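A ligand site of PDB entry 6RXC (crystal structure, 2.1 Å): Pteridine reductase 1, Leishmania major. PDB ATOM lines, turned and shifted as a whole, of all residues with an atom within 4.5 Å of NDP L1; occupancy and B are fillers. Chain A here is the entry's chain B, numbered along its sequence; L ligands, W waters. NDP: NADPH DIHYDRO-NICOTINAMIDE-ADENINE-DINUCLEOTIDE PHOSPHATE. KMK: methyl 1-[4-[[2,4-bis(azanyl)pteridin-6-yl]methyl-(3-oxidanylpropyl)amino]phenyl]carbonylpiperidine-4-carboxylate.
Water W3 lies within hydrogen-bond range of O2N of NDP L1 (2.6 Å), N of Gly 22 (2.7 Å), ND2 of Asn 112 (2.9 Å) and O of Gly 16 (3.5 Å).
Water W2 bridges an oxygen (O2X) of NDP L1 and a ring nitrogen (ND1) of His 41.
Water W4 lies within hydrogen-bond range of an oxygen (O3D) of NDP L1, the side-chain amino group of Lys 201, the backbone carbonyl oxygen of Met 182 and the backbone carbonyl oxygen of Ala 113.
Water W1 bridges O1X of NDP L1 and O of His 39.
Water W7 bridges OD2 of Asp 145 and N7A of NDP L1.
An oxygen (O2D) of NDP L1 is in hydrogen-bond range of a nitrogen (N3) of KMK L2, 2.6 Å away.
A nitrogen (N6A) of NDP L1 lies within hydrogen-bond range of the side-chain carboxylate (OD1) of Asp 145.
The guanidinium group of Arg 20 lies within salt-bridge range of an oxygen (O1N) of NDP L1.
N of His 41 sits at hydrogen-bond distance from O1X of NDP L1, 2.7 Å away.
N of Arg 42 lies within hydrogen-bond range of O2X of NDP L1 (2.8 Å).
An oxygen (O3D) of NDP L1 sits at hydrogen-bond distance from the backbone carbonyl oxygen (O) of Asn 112 (2.8 Å).
N of Ser 43 is in hydrogen-bond range of O1X of NDP L1, at 3.2 Å.
The side-chain hydroxyl (OG) of Ser 43 is in hydrogen-bond range of an oxygen (O3X) of NDP L1 (2.9 Å).
O2D of NDP L1 is in hydrogen-bond range of NZ of Lys 201.
The backbone NH (N) of Ser 230 lies within hydrogen-bond range of an oxygen (O7N) of NDP L1 (3.0 Å).
O of Ser 230 lies within hydrogen-bond range of N7N of NDP L1 (3.1 Å).
The backbone NH (N) of Leu 69 is in hydrogen-bond range of a nitrogen (N1A) of NDP L1.
O4B of NDP L1 is in hydrogen-bond range of N of Ser 114 (3.2 Å).
OG of Ser 114 lies within hydrogen-bond range of O2D of NDP L1.
The backbone NH (N) of Leu 21 sits at hydrogen-bond distance from an oxygen (O2N) of NDP L1, 3.3 Å away.
N2 of KMK L2 is in hydrogen-bond range of O of Ser 114, 2.8 Å away.
OG of Ser 114 sits at hydrogen-bond distance from N2 of KMK L2 (2.7 Å).
The side-chain hydroxyl (OH) of Tyr 197 sits at hydrogen-bond distance from a nitrogen (N4) of KMK L2.
The side-chain carboxylate (OD1) of Asp 68 lies close to a nitrogen (N1A) of NDP L1 (3.5 Å).
CA of Gly 16 touches C4B of NDP L1, 3.9 Å away.
His 39 touches NDP L1.
Tyr 40 touches NDP L1 (CB to O1X, 3.4 Å).
Ala 67 touches NDP L1.
Ser 70 touches NDP L1 (N to N6A, 3.7 Å).
Ala 113 touches NDP L1 (CA to O4B, 3.4 Å).
CB of Ser 115 touches N7A of NDP L1, at 3.4 Å.
CB of Met 182 touches O3D of NDP L1 (3.5 Å).
Val 183 touches NDP L1 (O to C6N, 3.3 Å).
Asp 184 touches NDP L1 (OD2 to C5N, 3.4 Å).
Tyr 197 touches NDP L1 (OH to O2D, 3.7 Å).
Pro 227 touches NDP L1.
Gly 228 touches NDP L1.
Leu 229 touches NDP L1 (C to O7N, 3.9 Å).
The backbone carbonyl oxygen (O) of Asp 145 lies within hydrogen-bond range of the side-chain hydroxyl (OG) of Ser 115, 3.3 Å away.
The side-chain hydroxyl of Ser 70 sits close to the backbone NH of Asp 145.
The side-chain hydroxyl (OG) of Ser 149 sits at hydrogen-bond distance from the backbone carbonyl oxygen (O) of Asp 145.
ND2 of Asn 112 sits at hydrogen-bond distance from O of Gly 16, at 3.0 Å.
OG of Ser 114 lies close to ND2 of Asn 150, 3.3 Å away.
The side-chain hydroxyl (OG) of Ser 149 sits at hydrogen-bond distance from the side-chain hydroxyl (OG) of Ser 115.
NE2 of His 39 sits at hydrogen-bond distance from O of Ala 67 (2.8 Å).
A ring nitrogen (ND1) of His 39 sits at hydrogen-bond distance from the backbone NH (N) of Gly 16 (3.2 Å).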
ATOM      1  N   GLY A  16     -23.400 -19.738  19.734  1.00  0.00           N
ATOM      2  CA  GLY A  16     -24.170 -20.970  19.695  1.00  0.00           C
ATOM      3  C   GLY A  16     -25.593 -20.787  20.177  1.00  0.00           C
ATOM      4  O   GLY A  16     -26.035 -21.584  20.999  1.00  0.00           O
ATOM      5  N   ARG A  20     -31.067 -25.534  22.172  1.00  0.00           N
ATOM      6  CA  ARG A  20     -30.816 -25.923  23.546  1.00  0.00           C
ATOM      7  C   ARG A  20     -30.524 -24.671  24.381  1.00  0.00           C
ATOM      8  O   ARG A  20     -31.222 -23.663  24.252  1.00  0.00           O
ATOM      9  CB  ARG A  20     -29.781 -27.049  23.521  1.00  0.00           C
ATOM     10  CG  ARG A  20     -30.334 -28.343  22.925  1.00  0.00           C
ATOM     11  CD  ARG A  20     -29.231 -29.225  22.359  1.00  0.00           C
ATOM     12  NE  ARG A  20     -28.170 -29.409  23.344  1.00  0.00           N
ATOM     13  CZ  ARG A  20     -28.239 -30.312  24.321  1.00  0.00           C
ATOM     14  NH1 ARG A  20     -29.300 -31.091  24.380  1.00  0.00           N
ATOM     15  NH2 ARG A  20     -27.263 -30.440  25.214  1.00  0.00           N
ATOM     16  N   LEU A  21     -29.453 -24.741  25.198  1.00  0.00           N
ATOM     17  CA  LEU A  21     -29.206 -23.777  26.258  1.00  0.00           C
ATOM     18  C   LEU A  21     -28.973 -22.385  25.656  1.00  0.00           C
ATOM     19  O   LEU A  21     -29.485 -21.390  26.185  1.00  0.00           O
ATOM     20  CB  LEU A  21     -27.975 -24.196  27.070  1.00  0.00           C
ATOM     21  CG  LEU A  21     -27.989 -25.495  27.879  1.00  0.00           C
ATOM     22  CD1 LEU A  21     -27.222 -25.279  29.187  1.00  0.00           C
ATOM     23  CD2 LEU A  21     -29.382 -25.983  28.174  1.00  0.00           C
ATOM     24  N   GLY A  22     -28.248 -22.308  24.545  1.00  0.00           N
ATOM     25  CA  GLY A  22     -28.010 -20.988  23.972  1.00  0.00           C
ATOM     26  C   GLY A  22     -29.280 -20.333  23.419  1.00  0.00           C
ATOM     27  O   GLY A  22     -29.383 -19.112  23.383  1.00  0.00           O
ATOM     28  N   HIS A  39     -25.551 -15.890  17.246  1.00  0.00           N
ATOM     29  CA  HIS A  39     -24.424 -16.526  16.563  1.00  0.00           C
ATOM     30  C   HIS A  39     -24.769 -17.993  16.408  1.00  0.00           C
ATOM     31  O   HIS A  39     -25.467 -18.539  17.256  1.00  0.00           O
ATOM     32  CB  HIS A  39     -23.037 -16.245  17.188  1.00  0.00           C
ATOM     33  CG  HIS A  39     -22.002 -17.214  16.704  1.00  0.00           C
ATOM     34  ND1 HIS A  39     -21.928 -18.527  17.173  1.00  0.00           N
ATOM     35  CD2 HIS A  39     -21.098 -17.102  15.694  1.00  0.00           C
ATOM     36  CE1 HIS A  39     -20.992 -19.174  16.490  1.00  0.00           C
ATOM     37  NE2 HIS A  39     -20.462 -18.311  15.591  1.00  0.00           N
ATOM     38  N   TYR A  40     -24.321 -18.576  15.279  1.00  0.00           N
ATOM     39  CA  TYR A  40     -24.451 -19.991  15.007  1.00  0.00           C
ATOM     40  C   TYR A  40     -23.309 -20.360  14.069  1.00  0.00           C
ATOM     41  O   TYR A  40     -22.681 -19.498  13.465  1.00  0.00           O
ATOM     42  CB  TYR A  40     -25.778 -20.340  14.311  1.00  0.00           C
ATOM     43  CG  TYR A  40     -25.860 -19.770  12.928  1.00  0.00           C
ATOM     44  CD1 TYR A  40     -26.181 -18.430  12.705  1.00  0.00           C
ATOM     45  CD2 TYR A  40     -25.522 -20.544  11.834  1.00  0.00           C
ATOM     46  CE1 TYR A  40     -26.214 -17.888  11.437  1.00  0.00           C
ATOM     47  CE2 TYR A  40     -25.516 -20.009  10.555  1.00  0.00           C
ATOM     48  CZ  TYR A  40     -25.886 -18.683  10.350  1.00  0.00           C
ATOM     49  OH  TYR A  40     -25.947 -18.196   9.072  1.00  0.00           O
ATOM     50  N   HIS A  41     -23.108 -21.660  13.941  1.00  0.00           N
ATOM     51  CA  HIS A  41     -22.077 -22.164  13.052  1.00  0.00           C
ATOM     52  C   HIS A  41     -22.762 -23.001  11.976  1.00  0.00           C
ATOM     53  O   HIS A  41     -22.860 -22.548  10.832  1.00  0.00           O
ATOM     54  CB  HIS A  41     -20.962 -22.852  13.884  1.00  0.00           C
ATOM     55  CG  HIS A  41     -19.921 -23.565  13.071  1.00  0.00           C
ATOM     56  ND1 HIS A  41     -19.694 -24.933  13.174  1.00  0.00           N
ATOM     57  CD2 HIS A  41     -19.050 -23.109  12.140  1.00  0.00           C
ATOM     58  CE1 HIS A  41     -18.709 -25.285  12.362  1.00  0.00           C
ATOM     59  NE2 HIS A  41     -18.309 -24.176  11.709  1.00  0.00           N
ATOM     60  N   ARG A  42     -23.288 -24.180  12.376  1.00  0.00           N
ATOM     61  CA  ARG A  42     -23.858 -25.109  11.409  1.00  0.00           C
ATOM     62  C   ARG A  42     -25.375 -24.975  11.326  1.00  0.00           C
ATOM     63  O   ARG A  42     -25.928 -25.178  10.261  1.00  0.00           O
ATOM     64  CB  ARG A  42     -23.401 -26.557  11.631  1.00  0.00           C
ATOM     65  CG  ARG A  42     -21.888 -26.706  11.588  1.00  0.00           C
ATOM     66  CD  ARG A  42     -21.429 -28.009  11.010  1.00  0.00           C
ATOM     67  NE  ARG A  42     -20.011 -27.877  10.747  1.00  0.00           N
ATOM     68  CZ  ARG A  42     -19.479 -27.310   9.670  1.00  0.00           C
ATOM     69  NH1 ARG A  42     -20.244 -26.820   8.703  1.00  0.00           N
ATOM     70  NH2 ARG A  42     -18.167 -27.247   9.552  1.00  0.00           N
ATOM     71  N   SER A  43     -26.038 -24.586  12.421  1.00  0.00           N
ATOM     72  CA  SER A  43     -27.492 -24.651  12.492  1.00  0.00           C
ATOM     73  C   SER A  43     -28.121 -23.350  11.990  1.00  0.00           C
ATOM     74  O   SER A  43     -28.764 -22.634  12.763  1.00  0.00           O
ATOM     75  CB  SER A  43     -27.977 -24.973  13.892  1.00  0.00           C
ATOM     76  OG  SER A  43     -27.603 -26.280  14.305  1.00  0.00           O
ATOM     77  N   ALA A  67     -20.306 -17.904  12.079  1.00  0.00           N
ATOM     78  CA  ALA A  67     -18.868 -18.007  12.132  1.00  0.00           C
ATOM     79  C   ALA A  67     -18.548 -19.365  12.747  1.00  0.00           C
ATOM     80  O   ALA A  67     -19.284 -19.911  13.574  1.00  0.00           O
ATOM     81  CB  ALA A  67     -18.205 -16.865  12.905  1.00  0.00           C
ATOM     82  N   ASP A  68     -17.432 -19.870  12.283  1.00  0.00           N
ATOM     83  CA  ASP A  68     -16.792 -20.995  12.930  1.00  0.00           C
ATOM     84  C   ASP A  68     -15.876 -20.387  13.994  1.00  0.00           C
ATOM     85  O   ASP A  68     -15.004 -19.600  13.679  1.00  0.00           O
ATOM     86  CB  ASP A  68     -16.109 -21.846  11.851  1.00  0.00           C
ATOM     87  CG  ASP A  68     -15.168 -22.880  12.446  1.00  0.00           C
ATOM     88  OD1 ASP A  68     -15.302 -23.171  13.682  1.00  0.00           O
ATOM     89  OD2 ASP A  68     -14.315 -23.387  11.676  1.00  0.00           O
ATOM     90  N   LEU A  69     -16.077 -20.777  15.249  1.00  0.00           N
ATOM     91  CA  LEU A  69     -15.192 -20.361  16.328  1.00  0.00           C
ATOM     92  C   LEU A  69     -14.056 -21.362  16.604  1.00  0.00           C
ATOM     93  O   LEU A  69     -13.237 -21.141  17.491  1.00  0.00           O
ATOM     94  CB  LEU A  69     -16.020 -20.147  17.589  1.00  0.00           C
ATOM     95  CG  LEU A  69     -17.139 -19.111  17.475  1.00  0.00           C
ATOM     96  CD1 LEU A  69     -17.874 -18.973  18.819  1.00  0.00           C
ATOM     97  CD2 LEU A  69     -16.568 -17.781  17.001  1.00  0.00           C
ATOM     98  N   SER A  70     -13.950 -22.438  15.829  1.00  0.00           N
ATOM     99  CA  SER A  70     -12.707 -23.215  15.832  1.00  0.00           C
ATOM    100  C   SER A  70     -11.423 -22.360  15.596  1.00  0.00           C
ATOM    101  O   SER A  70     -11.482 -21.313  14.902  1.00  0.00           O
ATOM    102  CB  SER A  70     -12.892 -24.298  14.856  1.00  0.00           C
ATOM    103  OG  SER A  70     -11.745 -25.106  14.801  1.00  0.00           O
ATOM    104  N   ASN A 112     -21.386 -19.074  24.877  1.00  0.00           N
ATOM    105  CA  ASN A 112     -22.069 -20.321  25.119  1.00  0.00           C
ATOM    106  C   ASN A 112     -21.605 -21.430  24.178  1.00  0.00           C
ATOM    107  O   ASN A 112     -21.734 -22.599  24.517  1.00  0.00           O
ATOM    108  CB  ASN A 112     -23.562 -20.023  24.988  1.00  0.00           C
ATOM    109  CG  ASN A 112     -24.384 -21.267  24.924  1.00  0.00           C
ATOM    110  OD1 ASN A 112     -24.700 -21.864  25.953  1.00  0.00           O
ATOM    111  ND2 ASN A 112     -24.715 -21.664  23.712  1.00  0.00           N
ATOM    112  N   ALA A 113     -21.179 -21.088  22.949  1.00  0.00           N
ATOM    113  CA  ALA A 113     -20.884 -22.092  21.938  1.00  0.00           C
ATOM    114  C   ALA A 113     -19.788 -23.006  22.486  1.00  0.00           C
ATOM    115  O   ALA A 113     -18.884 -22.523  23.190  1.00  0.00           O
ATOM    116  CB  ALA A 113     -20.414 -21.381  20.695  1.00  0.00           C
ATOM    117  N   SER A 114     -19.894 -24.324  22.245  1.00  0.00           N
ATOM    118  CA  SER A 114     -18.864 -25.236  22.766  1.00  0.00           C
ATOM    119  C   SER A 114     -19.010 -26.537  22.039  1.00  0.00           C
ATOM    120  O   SER A 114     -20.106 -27.083  21.975  1.00  0.00           O
ATOM    121  CB  SER A 114     -19.008 -25.483  24.269  1.00  0.00           C
ATOM    122  OG  SER A 114     -18.295 -26.639  24.686  1.00  0.00           O
ATOM    123  N   SER A 115     -17.929 -27.020  21.433  1.00  0.00           N
ATOM    124  CA  SER A 115     -18.001 -28.375  20.920  1.00  0.00           C
ATOM    125  C   SER A 115     -17.600 -29.273  22.083  1.00  0.00           C
ATOM    126  O   SER A 115     -16.936 -28.840  23.032  1.00  0.00           O
ATOM    127  CB  SER A 115     -17.105 -28.552  19.740  1.00  0.00           C
ATOM    128  OG  SER A 115     -15.854 -27.904  20.004  1.00  0.00           O
ATOM    129  N   ASP A 145     -10.683 -27.185  17.339  1.00  0.00           N
ATOM    130  CA  ASP A 145     -12.123 -27.045  17.546  1.00  0.00           C
ATOM    131  C   ASP A 145     -12.470 -26.919  19.023  1.00  0.00           C
ATOM    132  O   ASP A 145     -13.240 -26.054  19.407  1.00  0.00           O
ATOM    133  CB  ASP A 145     -12.878 -28.130  16.793  1.00  0.00           C
ATOM    134  CG  ASP A 145     -14.406 -28.096  16.879  1.00  0.00           C
ATOM    135  OD1 ASP A 145     -14.981 -26.975  16.880  1.00  0.00           O
ATOM    136  OD2 ASP A 145     -15.023 -29.188  16.969  1.00  0.00           O
ATOM    137  N   SER A 149     -13.319 -23.071  20.417  1.00  0.00           N
ATOM    138  CA  SER A 149     -14.669 -22.724  20.698  1.00  0.00           C
ATOM    139  C   SER A 149     -14.865 -22.467  22.200  1.00  0.00           C
ATOM    140  O   SER A 149     -15.554 -21.526  22.588  1.00  0.00           O
ATOM    141  CB  SER A 149     -15.546 -23.855  20.211  1.00  0.00           C
ATOM    142  OG  SER A 149     -15.435 -24.940  21.093  1.00  0.00           O
ATOM    143  N   ASN A 150     -14.158 -23.241  23.046  1.00  0.00           N
ATOM    144  CA  ASN A 150     -14.402 -23.249  24.482  1.00  0.00           C
ATOM    145  C   ASN A 150     -13.642 -22.138  25.134  1.00  0.00           C
ATOM    146  O   ASN A 150     -14.099 -21.673  26.203  1.00  0.00           O
ATOM    147  CB  ASN A 150     -14.151 -24.614  25.109  1.00  0.00           C
ATOM    148  CG  ASN A 150     -15.302 -25.551  24.796  1.00  0.00           C
ATOM    149  OD1 ASN A 150     -16.414 -25.344  25.268  1.00  0.00           O
ATOM    150  ND2 ASN A 150     -15.059 -26.631  24.057  1.00  0.00           N
ATOM    151  N   MET A 182     -20.032 -19.835  29.681  1.00  0.00           N
ATOM    152  CA  MET A 182     -20.639 -21.091  30.077  1.00  0.00           C
ATOM    153  C   MET A 182     -19.505 -22.089  30.301  1.00  0.00           C
ATOM    154  O   MET A 182     -18.767 -22.432  29.372  1.00  0.00           O
ATOM    155  CB  MET A 182     -21.663 -21.664  29.068  1.00  0.00           C
ATOM    156  CG  MET A 182     -22.748 -20.626  28.601  1.00  0.00           C
ATOM    157  SD  MET A 182     -23.697 -20.058  30.053  1.00  0.00           S
ATOM    158  CE  MET A 182     -24.662 -21.550  30.313  1.00  0.00           C
ATOM    159  N   VAL A 183     -19.335 -22.436  31.572  1.00  0.00           N
ATOM    160  CA  VAL A 183     -18.271 -23.297  32.052  1.00  0.00           C
ATOM    161  C   VAL A 183     -19.004 -24.592  32.423  1.00  0.00           C
ATOM    162  O   VAL A 183     -20.051 -24.832  31.869  1.00  0.00           O
ATOM    163  CB  VAL A 183     -17.444 -22.649  33.178  1.00  0.00           C
ATOM    164  CG1 VAL A 183     -16.653 -21.398  32.664  1.00  0.00           C
ATOM    165  CG2 VAL A 183     -18.282 -22.197  34.364  1.00  0.00           C
ATOM    166  N   ASP A 184     -18.449 -25.441  33.257  1.00  0.00           N
ATOM    167  CA  ASP A 184     -19.054 -26.733  33.527  1.00  0.00           C
ATOM    168  C   ASP A 184     -18.918 -26.969  35.022  1.00  0.00           C
ATOM    169  O   ASP A 184     -17.823 -26.808  35.576  1.00  0.00           O
ATOM    170  CB  ASP A 184     -18.256 -27.718  32.690  1.00  0.00           C
ATOM    171  CG  ASP A 184     -18.712 -29.150  32.745  1.00  0.00           C
ATOM    172  OD1 ASP A 184     -19.113 -29.556  33.812  1.00  0.00           O
ATOM    173  OD2 ASP A 184     -18.663 -29.809  31.705  1.00  0.00           O
ATOM    174  N   TYR A 197     -11.558 -31.157  26.063  1.00  0.00           N
ATOM    175  CA  TYR A 197     -12.693 -30.391  26.543  1.00  0.00           C
ATOM    176  C   TYR A 197     -12.422 -29.891  27.992  1.00  0.00           C
ATOM    177  O   TYR A 197     -12.757 -28.778  28.356  1.00  0.00           O
ATOM    178  CB  TYR A 197     -13.995 -31.248  26.370  1.00  0.00           C
ATOM    179  CG  TYR A 197     -15.192 -30.683  27.094  1.00  0.00           C
ATOM    180  CD1 TYR A 197     -15.929 -29.621  26.585  1.00  0.00           C
ATOM    181  CD2 TYR A 197     -15.502 -31.115  28.370  1.00  0.00           C
ATOM    182  CE1 TYR A 197     -16.977 -29.072  27.296  1.00  0.00           C
ATOM    183  CE2 TYR A 197     -16.592 -30.635  29.067  1.00  0.00           C
ATOM    184  CZ  TYR A 197     -17.299 -29.573  28.555  1.00  0.00           C
ATOM    185  OH  TYR A 197     -18.299 -29.078  29.328  1.00  0.00           O
ATOM    186  N   LYS A 201     -12.379 -25.802  29.217  1.00  0.00           N
ATOM    187  CA  LYS A 201     -13.221 -25.275  30.313  1.00  0.00           C
ATOM    188  C   LYS A 201     -12.427 -24.663  31.480  1.00  0.00           C
ATOM    189  O   LYS A 201     -12.742 -23.563  31.963  1.00  0.00           O
ATOM    190  CB  LYS A 201     -14.128 -26.392  30.864  1.00  0.00           C
ATOM    191  CG  LYS A 201     -15.374 -26.685  30.006  1.00  0.00           C
ATOM    192  CD  LYS A 201     -16.030 -25.426  29.350  1.00  0.00           C
ATOM    193  CE  LYS A 201     -17.368 -25.755  28.673  1.00  0.00           C
ATOM    194  NZ  LYS A 201     -17.952 -24.652  27.864  1.00  0.00           N
ATOM    195  N   PRO A 227     -23.367 -25.394  34.170  1.00  0.00           N
ATOM    196  CA  PRO A 227     -24.329 -26.485  34.210  1.00  0.00           C
ATOM    197  C   PRO A 227     -23.688 -27.798  34.663  1.00  0.00           C
ATOM    198  O   PRO A 227     -22.491 -28.026  34.450  1.00  0.00           O
ATOM    199  CB  PRO A 227     -24.784 -26.620  32.750  1.00  0.00           C
ATOM    200  CG  PRO A 227     -24.474 -25.285  32.124  1.00  0.00           C
ATOM    201  CD  PRO A 227     -23.186 -24.836  32.814  1.00  0.00           C
ATOM    202  N   GLY A 228     -24.521 -28.671  35.265  1.00  0.00           N
ATOM    203  CA  GLY A 228     -24.162 -30.054  35.505  1.00  0.00           C
ATOM    204  C   GLY A 228     -24.662 -30.985  34.412  1.00  0.00           C
ATOM    205  O   GLY A 228     -23.933 -31.234  33.444  1.00  0.00           O
ATOM    206  N   LEU A 229     -25.782 -31.687  34.646  1.00  0.00           N
ATOM    207  CA  LEU A 229     -26.429 -32.447  33.573  1.00  0.00           C
ATOM    208  C   LEU A 229     -27.610 -31.579  33.124  1.00  0.00           C
ATOM    209  O   LEU A 229     -28.415 -31.218  33.974  1.00  0.00           O
ATOM    210  CB  LEU A 229     -26.905 -33.809  34.071  1.00  0.00           C
ATOM    211  CG  LEU A 229     -25.884 -34.736  34.765  1.00  0.00           C
ATOM    212  CD1 LEU A 229     -26.464 -36.105  35.018  1.00  0.00           C
ATOM    213  CD2 LEU A 229     -24.579 -34.887  33.952  1.00  0.00           C
ATOM    214  N   SER A 230     -27.644 -31.171  31.871  1.00  0.00           N
ATOM    215  CA  SER A 230     -28.704 -30.301  31.351  1.00  0.00           C
ATOM    216  C   SER A 230     -29.173 -30.752  29.966  1.00  0.00           C
ATOM    217  O   SER A 230     -28.338 -30.955  29.069  1.00  0.00           O
ATOM    218  CB  SER A 230     -28.287 -28.879  31.223  1.00  0.00           C
ATOM    219  OG  SER A 230     -28.001 -28.306  32.482  1.00  0.00           O
HETATM  220  PA  NDP L   1     -24.403 -27.840  22.613  1.00  0.00           P
HETATM  221  O1A NDP L   1     -23.638 -29.107  22.655  1.00  0.00           O
HETATM  222  O2A NDP L   1     -25.848 -28.006  22.277  1.00  0.00           O
HETATM  223  O5B NDP L   1     -23.742 -26.770  21.654  1.00  0.00           O
HETATM  224  C5B NDP L   1     -23.992 -25.372  21.670  1.00  0.00           C
HETATM  225  C4B NDP L   1     -23.675 -24.816  20.298  1.00  0.00           C
HETATM  226  O4B NDP L   1     -22.263 -24.583  20.151  1.00  0.00           O
HETATM  227  C3B NDP L   1     -23.964 -25.724  19.095  1.00  0.00           C
HETATM  228  O3B NDP L   1     -25.358 -25.780  18.799  1.00  0.00           O
HETATM  229  C2B NDP L   1     -23.085 -25.126  18.007  1.00  0.00           C
HETATM  230  O2B NDP L   1     -23.687 -24.182  17.114  1.00  0.00           O
HETATM  231  C1B NDP L   1     -22.001 -24.366  18.781  1.00  0.00           C
HETATM  232  N9A NDP L   1     -20.663 -24.786  18.400  1.00  0.00           N
HETATM  233  C8A NDP L   1     -20.086 -26.024  18.633  1.00  0.00           C
HETATM  234  N7A NDP L   1     -18.885 -26.103  18.117  1.00  0.00           N
HETATM  235  C5A NDP L   1     -18.672 -24.907  17.459  1.00  0.00           C
HETATM  236  C6A NDP L   1     -17.565 -24.414  16.717  1.00  0.00           C
HETATM  237  N6A NDP L   1     -16.459 -25.112  16.439  1.00  0.00           N
HETATM  238  N1A NDP L   1     -17.701 -23.155  16.198  1.00  0.00           N
HETATM  239  C2A NDP L   1     -18.811 -22.449  16.465  1.00  0.00           C
HETATM  240  N3A NDP L   1     -19.903 -22.819  17.134  1.00  0.00           N
HETATM  241  C4A NDP L   1     -19.766 -24.083  17.622  1.00  0.00           C
HETATM  242  O3  NDP L   1     -24.334 -27.176  24.099  1.00  0.00           O
HETATM  243  PN  NDP L   1     -25.432 -27.102  25.283  1.00  0.00           P
HETATM  244  O1N NDP L   1     -25.737 -28.484  25.711  1.00  0.00           O
HETATM  245  O2N NDP L   1     -26.476 -26.204  24.758  1.00  0.00           O
HETATM  246  O5D NDP L   1     -24.598 -26.365  26.476  1.00  0.00           O
HETATM  247  C5D NDP L   1     -24.307 -24.962  26.355  1.00  0.00           C
HETATM  248  C4D NDP L   1     -23.077 -24.536  27.122  1.00  0.00           C
HETATM  249  O4D NDP L   1     -23.103 -25.033  28.480  1.00  0.00           O
HETATM  250  C3D NDP L   1     -21.742 -25.017  26.521  1.00  0.00           C
HETATM  251  O3D NDP L   1     -20.716 -24.052  26.729  1.00  0.00           O
HETATM  252  C2D NDP L   1     -21.505 -26.277  27.325  1.00  0.00           C
HETATM  253  O2D NDP L   1     -20.138 -26.576  27.350  1.00  0.00           O
HETATM  254  C1D NDP L   1     -21.983 -25.826  28.698  1.00  0.00           C
HETATM  255  N1N NDP L   1     -22.417 -27.010  29.474  1.00  0.00           N
HETATM  256  C2N NDP L   1     -23.511 -27.748  29.133  1.00  0.00           C
HETATM  257  C3N NDP L   1     -23.753 -28.984  29.730  1.00  0.00           C
HETATM  258  C7N NDP L   1     -25.000 -29.783  29.377  1.00  0.00           C
HETATM  259  O7N NDP L   1     -25.288 -30.767  30.066  1.00  0.00           O
HETATM  260  N7N NDP L   1     -25.797 -29.383  28.388  1.00  0.00           N
HETATM  261  C4N NDP L   1     -22.789 -29.514  30.736  1.00  0.00           C
HETATM  262  C5N NDP L   1     -21.769 -28.567  31.160  1.00  0.00           C
HETATM  263  C6N NDP L   1     -21.566 -27.434  30.507  1.00  0.00           C
HETATM  264  P2B NDP L   1     -24.252 -24.770  15.688  1.00  0.00           P
HETATM  265  O1X NDP L   1     -24.760 -23.496  15.113  1.00  0.00           O
HETATM  266  O2X NDP L   1     -23.113 -25.407  14.872  1.00  0.00           O
HETATM  267  O3X NDP L   1     -25.316 -25.848  16.064  1.00  0.00           O
HETATM  268  C2  KMK L   2     -21.178 -28.990  25.336  1.00  0.00           C
HETATM  269  C7  KMK L   2     -24.080 -32.640  26.058  1.00  0.00           C
HETATM  270  C4  KMK L   2     -21.172 -30.006  27.466  1.00  0.00           C
HETATM  271  C6  KMK L   2     -23.621 -32.775  27.394  1.00  0.00           C
HETATM  272  CBG KMK L   2     -23.989 -46.745  27.689  1.00  0.00           C
HETATM  273  OBE KMK L   2     -23.338 -45.528  28.068  1.00  0.00           O
HETATM  274  CBD KMK L   2     -23.408 -44.478  27.165  1.00  0.00           C
HETATM  275  OBF KMK L   2     -24.444 -44.226  26.541  1.00  0.00           O
HETATM  276  CAZ KMK L   2     -22.085 -43.610  26.950  1.00  0.00           C
HETATM  277  CBA KMK L   2     -22.107 -42.939  25.515  1.00  0.00           C
HETATM  278  CAV KMK L   2     -21.161 -41.772  25.380  1.00  0.00           C
HETATM  279  CAY KMK L   2     -21.752 -42.627  28.188  1.00  0.00           C
HETATM  280  CAX KMK L   2     -21.192 -41.182  27.850  1.00  0.00           C
HETATM  281  NAW KMK L   2     -21.459 -40.735  26.434  1.00  0.00           N
HETATM  282  CBB KMK L   2     -21.952 -39.525  26.016  1.00  0.00           C
HETATM  283  OBC KMK L   2     -22.125 -39.350  24.798  1.00  0.00           O
HETATM  284  CAU KMK L   2     -22.259 -38.400  26.864  1.00  0.00           C
HETATM  285  CAT KMK L   2     -22.919 -37.313  26.262  1.00  0.00           C
HETATM  286  CAO KMK L   2     -23.270 -36.150  26.945  1.00  0.00           C
HETATM  287  CAQ KMK L   2     -21.939 -38.243  28.228  1.00  0.00           C
HETATM  288  CAR KMK L   2     -22.333 -37.066  28.911  1.00  0.00           C
HETATM  289  CAS KMK L   2     -22.970 -35.972  28.305  1.00  0.00           C
HETATM  290  N10 KMK L   2     -23.334 -34.785  28.903  1.00  0.00           N
HETATM  291  CAP KMK L   2     -23.058 -34.332  30.299  1.00  0.00           C
HETATM  292  CBH KMK L   2     -21.826 -34.937  31.000  1.00  0.00           C
HETATM  293  CBI KMK L   2     -20.780 -33.875  31.394  1.00  0.00           C
HETATM  294  OBJ KMK L   2     -20.298 -34.126  32.793  1.00  0.00           O
HETATM  295  C9  KMK L   2     -24.228 -33.824  28.202  1.00  0.00           C
HETATM  296  N5  KMK L   2     -22.675 -31.905  27.836  1.00  0.00           N
HETATM  297  C4A KMK L   2     -22.165 -30.932  27.029  1.00  0.00           C
HETATM  298  N4  KMK L   2     -20.661 -30.059  28.695  1.00  0.00           N
HETATM  299  N3  KMK L   2     -20.734 -29.060  26.650  1.00  0.00           N
HETATM  300  N2  KMK L   2     -20.627 -28.036  24.591  1.00  0.00           N
HETATM  301  N1  KMK L   2     -22.135 -29.837  24.850  1.00  0.00           N
HETATM  302  C8A KMK L   2     -22.625 -30.789  25.673  1.00  0.00           C
HETATM  303  N8  KMK L   2     -23.583 -31.645  25.218  1.00  0.00           N
HETATM  304  O   HOH W   1     -25.958 -21.829  17.355  1.00  0.00           O
HETATM  305  O   HOH W   2     -20.863 -26.697  15.356  1.00  0.00           O
HETATM  306  O   HOH W   3     -26.471 -23.996  23.438  1.00  0.00           O
HETATM  307  O   HOH W   4     -18.582 -22.312  26.363  1.00  0.00           O
HETATM  308  O   HOH W   5     -22.141 -31.967  21.878  1.00  0.00           O
HETATM  309  O   HOH W   6     -25.315 -28.319  16.660  1.00  0.00           O
HETATM  310  O   HOH W   7     -17.564 -28.564  16.297  1.00  0.00           O
HETATM  311  O   HOH W   8     -23.077 -28.278  15.377  1.00  0.00           O
